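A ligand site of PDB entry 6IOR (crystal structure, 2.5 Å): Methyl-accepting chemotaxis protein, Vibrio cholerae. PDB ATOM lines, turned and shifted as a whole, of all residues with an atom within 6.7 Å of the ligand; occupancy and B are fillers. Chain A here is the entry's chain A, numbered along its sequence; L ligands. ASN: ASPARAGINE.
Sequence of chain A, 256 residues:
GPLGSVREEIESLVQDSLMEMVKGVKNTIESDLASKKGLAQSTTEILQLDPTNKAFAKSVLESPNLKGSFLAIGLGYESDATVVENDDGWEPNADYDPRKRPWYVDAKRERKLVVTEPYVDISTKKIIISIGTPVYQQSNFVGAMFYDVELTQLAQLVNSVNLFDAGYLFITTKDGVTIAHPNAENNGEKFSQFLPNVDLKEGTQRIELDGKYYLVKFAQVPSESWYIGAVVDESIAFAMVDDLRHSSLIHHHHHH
The side-chain hydroxyl (OH) of Tyr 119 sits at hydrogen-bond distance from a nitrogen (N) of the ligand, at 3.0 Å. OXT of the ligand sits at hydrogen-bond distance from OH of Tyr 96, at 3.0 Å. The indole nitrogen (NE1) of Trp 103 sits at hydrogen-bond distance from an oxygen (OXT) of the ligand (3.1 Å). The guanidinium group (NE) of Arg 101 lies within salt-bridge range of an oxygen (OXT) of the ligand. OD1 of Asp 121 is in salt-bridge range of N of the ligand, 3.0 Å away. The backbone NH of Ile 122 lies within hydrogen-bond range of an oxygen (O) of the ligand (3.3 Å). OD2 of Asp 148 is in salt-bridge range of N of the ligand.
The side-chain hydroxyl of Thr 124 is in hydrogen-bond range of the side-chain carboxylate of Asp 121, 2.6 Å away. OG of Ser 123 is in hydrogen-bond range of OD2 of Asp 87, at 3.2 Å. The side-chain hydroxyl of Tyr 119 lies within hydrogen-bond range of the side-chain hydroxyl of Ser 130 (2.5 Å). N of Asp 148 lies within hydrogen-bond range of O of Ala 72 (2.9 Å). OD1 of Asp 121 lies within hydrogen-bond range of N of Ser 123, 3.3 Å away. O of Tyr 119 lies within hydrogen-bond range of N of Ile 128, at 2.9 Å. The side-chain carboxylate (OD1) of Asp 148 is in hydrogen-bond range of the side-chain hydroxyl (OG) of Ser 130 (2.7 Å).
Residues that only touch the ligand: Trp 90, Ser 123, Ile 128 and Phe 146. Of the 21 residues printed, 11 come within 4 Å of the ligand.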
ATOM      1  N   ALA A  72     -31.667  25.066  -5.795  1.00  0.00           N
ATOM      2  CA  ALA A  72     -31.939  23.656  -6.046  1.00  0.00           C
ATOM      3  C   ALA A  72     -30.653  22.877  -5.788  1.00  0.00           C
ATOM      4  O   ALA A  72     -29.566  23.427  -5.870  1.00  0.00           O
ATOM      5  CB  ALA A  72     -32.434  23.420  -7.477  1.00  0.00           C
ATOM      6  N   ILE A  73     -30.799  21.600  -5.474  1.00  0.00           N
ATOM      7  CA  ILE A  73     -29.676  20.693  -5.289  1.00  0.00           C
ATOM      8  C   ILE A  73     -29.947  19.364  -6.025  1.00  0.00           C
ATOM      9  O   ILE A  73     -31.090  18.920  -6.107  1.00  0.00           O
ATOM     10  CB  ILE A  73     -29.428  20.391  -3.798  1.00  0.00           C
ATOM     11  CG1 ILE A  73     -29.492  21.673  -2.962  1.00  0.00           C
ATOM     12  CG2 ILE A  73     -28.133  19.600  -3.601  1.00  0.00           C
ATOM     13  CD1 ILE A  73     -29.555  21.439  -1.473  1.00  0.00           C
ATOM     14  N   GLU A  85     -32.995  14.857  -7.362  1.00  0.00           N
ATOM     15  CA  GLU A  85     -33.017  16.303  -7.088  1.00  0.00           C
ATOM     16  C   GLU A  85     -34.239  16.759  -6.304  1.00  0.00           C
ATOM     17  O   GLU A  85     -35.218  16.031  -6.192  1.00  0.00           O
ATOM     18  CB  GLU A  85     -32.903  17.089  -8.402  1.00  0.00           C
ATOM     19  CG  GLU A  85     -33.835  16.632  -9.530  1.00  0.00           C
ATOM     20  CD  GLU A  85     -35.274  16.979  -9.281  1.00  0.00           C
ATOM     21  OE1 GLU A  85     -36.141  16.136  -9.552  1.00  0.00           O
ATOM     22  OE2 GLU A  85     -35.559  18.105  -8.819  1.00  0.00           O
ATOM     23  N   ASP A  87     -36.001  19.906  -6.646  1.00  0.00           N
ATOM     24  CA  ASP A  87     -36.699  21.023  -7.264  1.00  0.00           C
ATOM     25  C   ASP A  87     -38.141  20.582  -7.470  1.00  0.00           C
ATOM     26  O   ASP A  87     -38.418  19.678  -8.275  1.00  0.00           O
ATOM     27  CB  ASP A  87     -36.021  21.409  -8.580  1.00  0.00           C
ATOM     28  CG  ASP A  87     -36.472  22.762  -9.125  1.00  0.00           C
ATOM     29  OD1 ASP A  87     -37.581  23.243  -8.795  1.00  0.00           O
ATOM     30  OD2 ASP A  87     -35.698  23.346  -9.933  1.00  0.00           O
ATOM     31  N   TRP A  90     -39.467  21.310 -11.130  1.00  0.00           N
ATOM     32  CA  TRP A  90     -38.706  20.876 -12.307  1.00  0.00           C
ATOM     33  C   TRP A  90     -38.441  19.378 -12.300  1.00  0.00           C
ATOM     34  O   TRP A  90     -38.188  18.784 -11.254  1.00  0.00           O
ATOM     35  CB  TRP A  90     -37.372  21.621 -12.393  1.00  0.00           C
ATOM     36  CG  TRP A  90     -36.485  21.158 -13.535  1.00  0.00           C
ATOM     37  CD1 TRP A  90     -36.611  21.496 -14.840  1.00  0.00           C
ATOM     38  CD2 TRP A  90     -35.334  20.295 -13.453  1.00  0.00           C
ATOM     39  NE1 TRP A  90     -35.626  20.894 -15.587  1.00  0.00           N
ATOM     40  CE2 TRP A  90     -34.826  20.161 -14.761  1.00  0.00           C
ATOM     41  CE3 TRP A  90     -34.688  19.630 -12.408  1.00  0.00           C
ATOM     42  CZ2 TRP A  90     -33.697  19.374 -15.061  1.00  0.00           C
ATOM     43  CZ3 TRP A  90     -33.567  18.855 -12.691  1.00  0.00           C
ATOM     44  CH2 TRP A  90     -33.084  18.735 -14.013  1.00  0.00           C
ATOM     45  N   TYR A  96     -32.040  15.552 -20.930  1.00  0.00           N
ATOM     46  CA  TYR A  96     -31.089  16.024 -19.919  1.00  0.00           C
ATOM     47  C   TYR A  96     -30.044  14.959 -19.588  1.00  0.00           C
ATOM     48  O   TYR A  96     -30.387  13.856 -19.204  1.00  0.00           O
ATOM     49  CB  TYR A  96     -31.835  16.457 -18.642  1.00  0.00           C
ATOM     50  CG  TYR A  96     -30.968  17.124 -17.593  1.00  0.00           C
ATOM     51  CD1 TYR A  96     -30.592  18.460 -17.722  1.00  0.00           C
ATOM     52  CD2 TYR A  96     -30.539  16.423 -16.454  1.00  0.00           C
ATOM     53  CE1 TYR A  96     -29.807  19.078 -16.767  1.00  0.00           C
ATOM     54  CE2 TYR A  96     -29.745  17.039 -15.495  1.00  0.00           C
ATOM     55  CZ  TYR A  96     -29.376  18.355 -15.660  1.00  0.00           C
ATOM     56  OH  TYR A  96     -28.583  18.991 -14.715  1.00  0.00           O
ATOM     57  N   PRO A  98     -26.898  14.841 -17.049  1.00  0.00           N
ATOM     58  CA  PRO A  98     -26.104  15.479 -15.979  1.00  0.00           C
ATOM     59  C   PRO A  98     -24.638  15.611 -16.341  1.00  0.00           C
ATOM     60  O   PRO A  98     -24.042  16.658 -16.087  1.00  0.00           O
ATOM     61  CB  PRO A  98     -26.277  14.528 -14.770  1.00  0.00           C
ATOM     62  CG  PRO A  98     -27.121  13.311 -15.309  1.00  0.00           C
ATOM     63  CD  PRO A  98     -27.861  13.856 -16.505  1.00  0.00           C
ATOM     64  N   ARG A 101     -23.304  18.729 -18.211  1.00  0.00           N
ATOM     65  CA  ARG A 101     -23.561  20.016 -17.569  1.00  0.00           C
ATOM     66  C   ARG A 101     -22.250  20.515 -16.937  1.00  0.00           C
ATOM     67  O   ARG A 101     -21.403  19.704 -16.578  1.00  0.00           O
ATOM     68  CB  ARG A 101     -24.688  19.896 -16.517  1.00  0.00           C
ATOM     69  CG  ARG A 101     -26.041  19.385 -17.033  1.00  0.00           C
ATOM     70  CD  ARG A 101     -26.605  20.279 -18.125  1.00  0.00           C
ATOM     71  NE  ARG A 101     -27.098  21.559 -17.641  1.00  0.00           N
ATOM     72  CZ  ARG A 101     -26.942  22.716 -18.300  1.00  0.00           C
ATOM     73  NH1 ARG A 101     -26.297  22.735 -19.461  1.00  0.00           N
ATOM     74  NH2 ARG A 101     -27.432  23.843 -17.799  1.00  0.00           N
ATOM     75  N   PRO A 102     -22.079  21.837 -16.821  1.00  0.00           N
ATOM     76  CA  PRO A 102     -20.787  22.406 -16.411  1.00  0.00           C
ATOM     77  C   PRO A 102     -20.412  22.124 -14.958  1.00  0.00           C
ATOM     78  O   PRO A 102     -19.219  21.957 -14.685  1.00  0.00           O
ATOM     79  CB  PRO A 102     -20.974  23.917 -16.641  1.00  0.00           C
ATOM     80  CG  PRO A 102     -22.451  24.136 -16.524  1.00  0.00           C
ATOM     81  CD  PRO A 102     -23.087  22.887 -17.075  1.00  0.00           C
ATOM     82  N   TRP A 103     -21.398  22.071 -14.066  1.00  0.00           N
ATOM     83  CA  TRP A 103     -21.138  21.735 -12.668  1.00  0.00           C
ATOM     84  C   TRP A 103     -20.497  20.354 -12.542  1.00  0.00           C
ATOM     85  O   TRP A 103     -19.684  20.105 -11.655  1.00  0.00           O
ATOM     86  CB  TRP A 103     -22.414  21.816 -11.818  1.00  0.00           C
ATOM     87  CG  TRP A 103     -23.615  21.049 -12.341  1.00  0.00           C
ATOM     88  CD1 TRP A 103     -24.630  21.544 -13.109  1.00  0.00           C
ATOM     89  CD2 TRP A 103     -23.942  19.678 -12.080  1.00  0.00           C
ATOM     90  NE1 TRP A 103     -25.547  20.556 -13.370  1.00  0.00           N
ATOM     91  CE2 TRP A 103     -25.164  19.396 -12.754  1.00  0.00           C
ATOM     92  CE3 TRP A 103     -23.320  18.645 -11.363  1.00  0.00           C
ATOM     93  CZ2 TRP A 103     -25.768  18.144 -12.731  1.00  0.00           C
ATOM     94  CZ3 TRP A 103     -23.927  17.373 -11.339  1.00  0.00           C
ATOM     95  CH2 TRP A 103     -25.137  17.140 -12.024  1.00  0.00           C
ATOM     96  N   TYR A 119     -23.614  30.654 -15.798  1.00  0.00           N
ATOM     97  CA  TYR A 119     -24.175  29.978 -16.970  1.00  0.00           C
ATOM     98  C   TYR A 119     -25.684  30.069 -16.891  1.00  0.00           C
ATOM     99  O   TYR A 119     -26.257  30.380 -15.840  1.00  0.00           O
ATOM    100  CB  TYR A 119     -23.711  28.488 -17.074  1.00  0.00           C
ATOM    101  CG  TYR A 119     -24.258  27.551 -15.996  1.00  0.00           C
ATOM    102  CD1 TYR A 119     -23.588  27.381 -14.784  1.00  0.00           C
ATOM    103  CD2 TYR A 119     -25.426  26.825 -16.211  1.00  0.00           C
ATOM    104  CE1 TYR A 119     -24.070  26.523 -13.805  1.00  0.00           C
ATOM    105  CE2 TYR A 119     -25.917  25.969 -15.237  1.00  0.00           C
ATOM    106  CZ  TYR A 119     -25.230  25.817 -14.029  1.00  0.00           C
ATOM    107  OH  TYR A 119     -25.729  24.961 -13.060  1.00  0.00           O
ATOM    108  N   VAL A 120     -26.335  29.792 -18.025  1.00  0.00           N
ATOM    109  CA  VAL A 120     -27.788  29.770 -18.121  1.00  0.00           C
ATOM    110  C   VAL A 120     -28.388  28.478 -17.524  1.00  0.00           C
ATOM    111  O   VAL A 120     -28.154  27.370 -18.015  1.00  0.00           O
ATOM    112  CB  VAL A 120     -28.242  29.892 -19.577  1.00  0.00           C
ATOM    113  CG1 VAL A 120     -29.757  29.819 -19.678  1.00  0.00           C
ATOM    114  CG2 VAL A 120     -27.661  31.166 -20.205  1.00  0.00           C
ATOM    115  N   ASP A 121     -29.163  28.659 -16.452  1.00  0.00           N
ATOM    116  CA  ASP A 121     -29.867  27.555 -15.805  1.00  0.00           C
ATOM    117  C   ASP A 121     -30.890  26.894 -16.756  1.00  0.00           C
ATOM    118  O   ASP A 121     -31.623  27.579 -17.463  1.00  0.00           O
ATOM    119  CB  ASP A 121     -30.565  28.092 -14.547  1.00  0.00           C
ATOM    120  CG  ASP A 121     -31.282  27.013 -13.784  1.00  0.00           C
ATOM    121  OD1 ASP A 121     -30.799  25.857 -13.775  1.00  0.00           O
ATOM    122  OD2 ASP A 121     -32.344  27.320 -13.184  1.00  0.00           O
ATOM    123  N   ILE A 122     -30.934  25.565 -16.770  1.00  0.00           N
ATOM    124  CA  ILE A 122     -31.956  24.876 -17.581  1.00  0.00           C
ATOM    125  C   ILE A 122     -33.350  24.970 -16.954  1.00  0.00           C
ATOM    126  O   ILE A 122     -34.345  25.038 -17.680  1.00  0.00           O
ATOM    127  CB  ILE A 122     -31.582  23.366 -17.821  1.00  0.00           C
ATOM    128  CG1 ILE A 122     -30.476  23.257 -18.872  1.00  0.00           C
ATOM    129  CG2 ILE A 122     -32.795  22.492 -18.204  1.00  0.00           C
ATOM    130  CD1 ILE A 122     -30.107  21.828 -19.146  1.00  0.00           C
ATOM    131  N   SER A 123     -33.425  24.978 -15.631  1.00  0.00           N
ATOM    132  CA  SER A 123     -34.732  25.000 -14.950  1.00  0.00           C
ATOM    133  C   SER A 123     -35.454  26.353 -15.083  1.00  0.00           C
ATOM    134  O   SER A 123     -36.618  26.412 -15.500  1.00  0.00           O
ATOM    135  CB  SER A 123     -34.553  24.627 -13.478  1.00  0.00           C
ATOM    136  OG  SER A 123     -35.747  24.866 -12.737  1.00  0.00           O
ATOM    137  N   THR A 124     -34.756  27.436 -14.732  1.00  0.00           N
ATOM    138  CA  THR A 124     -35.343  28.782 -14.691  1.00  0.00           C
ATOM    139  C   THR A 124     -34.926  29.686 -15.856  1.00  0.00           C
ATOM    140  O   THR A 124     -35.436  30.794 -15.976  1.00  0.00           O
ATOM    141  CB  THR A 124     -34.969  29.510 -13.374  1.00  0.00           C
ATOM    142  OG1 THR A 124     -33.543  29.647 -13.281  1.00  0.00           O
ATOM    143  CG2 THR A 124     -35.488  28.754 -12.152  1.00  0.00           C
ATOM    144  N   ILE A 128     -26.938  31.868 -13.477  1.00  0.00           N
ATOM    145  CA  ILE A 128     -26.650  31.477 -12.104  1.00  0.00           C
ATOM    146  C   ILE A 128     -25.234  30.988 -11.988  1.00  0.00           C
ATOM    147  O   ILE A 128     -24.496  30.977 -12.970  1.00  0.00           O
ATOM    148  CB  ILE A 128     -27.592  30.356 -11.614  1.00  0.00           C
ATOM    149  CG1 ILE A 128     -27.326  29.065 -12.399  1.00  0.00           C
ATOM    150  CG2 ILE A 128     -29.068  30.773 -11.721  1.00  0.00           C
ATOM    151  CD1 ILE A 128     -27.991  27.823 -11.819  1.00  0.00           C
ATOM    152  N   ILE A 129     -24.830  30.586 -10.790  1.00  0.00           N
ATOM    153  CA  ILE A 129     -23.624  29.797 -10.641  1.00  0.00           C
ATOM    154  C   ILE A 129     -24.005  28.597  -9.812  1.00  0.00           C
ATOM    155  O   ILE A 129     -25.051  28.598  -9.173  1.00  0.00           O
ATOM    156  CB  ILE A 129     -22.479  30.556  -9.953  1.00  0.00           C
ATOM    157  CG1 ILE A 129     -23.021  31.411  -8.793  1.00  0.00           C
ATOM    158  CG2 ILE A 129     -21.725  31.381 -10.955  1.00  0.00           C
ATOM    159  CD1 ILE A 129     -21.948  31.933  -7.824  1.00  0.00           C
ATOM    160  N   SER A 130     -23.151  27.575  -9.814  1.00  0.00           N
ATOM    161  CA  SER A 130     -23.398  26.384  -9.018  1.00  0.00           C
ATOM    162  C   SER A 130     -22.152  26.006  -8.264  1.00  0.00           C
ATOM    163  O   SER A 130     -21.018  26.227  -8.732  1.00  0.00           O
ATOM    164  CB  SER A 130     -23.869  25.205  -9.897  1.00  0.00           C
ATOM    165  OG  SER A 130     -24.954  25.577 -10.736  1.00  0.00           O
ATOM    166  N   PHE A 146     -24.773  19.310  -7.985  1.00  0.00           N
ATOM    167  CA  PHE A 146     -24.902  20.754  -8.108  1.00  0.00           C
ATOM    168  C   PHE A 146     -25.616  21.323  -6.897  1.00  0.00           C
ATOM    169  O   PHE A 146     -26.535  20.716  -6.356  1.00  0.00           O
ATOM    170  CB  PHE A 146     -25.663  21.149  -9.391  1.00  0.00           C
ATOM    171  CG  PHE A 146     -27.097  20.670  -9.431  1.00  0.00           C
ATOM    172  CD1 PHE A 146     -28.129  21.456  -8.909  1.00  0.00           C
ATOM    173  CD2 PHE A 146     -27.417  19.443  -9.987  1.00  0.00           C
ATOM    174  CE1 PHE A 146     -29.465  21.023  -8.947  1.00  0.00           C
ATOM    175  CE2 PHE A 146     -28.745  19.008 -10.043  1.00  0.00           C
ATOM    176  CZ  PHE A 146     -29.776  19.794  -9.521  1.00  0.00           C
ATOM    177  N   ASP A 148     -27.267  25.033  -6.578  1.00  0.00           N
ATOM    178  CA  ASP A 148     -27.473  26.223  -7.386  1.00  0.00           C
ATOM    179  C   ASP A 148     -27.592  27.453  -6.506  1.00  0.00           C
ATOM    180  O   ASP A 148     -28.312  27.472  -5.491  1.00  0.00           O
ATOM    181  CB  ASP A 148     -28.712  26.081  -8.288  1.00  0.00           C
ATOM    182  CG  ASP A 148     -28.488  25.123  -9.458  1.00  0.00           C
ATOM    183  OD1 ASP A 148     -27.310  24.785  -9.732  1.00  0.00           O
ATOM    184  OD2 ASP A 148     -29.477  24.715 -10.110  1.00  0.00           O
HETATM  185  N   ASN L   1     -28.565  24.151 -12.592  1.00  0.00           N
HETATM  186  CA  ASN L   1     -28.275  22.811 -13.098  1.00  0.00           C
HETATM  187  C   ASN L   1     -28.207  22.801 -14.640  1.00  0.00           C
HETATM  188  O   ASN L   1     -28.651  23.767 -15.279  1.00  0.00           O
HETATM  189  CB  ASN L   1     -29.333  21.820 -12.592  1.00  0.00           C
HETATM  190  CG  ASN L   1     -30.757  22.234 -12.966  1.00  0.00           C
HETATM  191  OD1 ASN L   1     -30.984  22.753 -14.059  1.00  0.00           O
HETATM  192  ND2 ASN L   1     -31.715  22.035 -12.056  1.00  0.00           N
HETATM  193  OXT ASN L   1     -27.699  21.860 -15.252  1.00  0.00           O
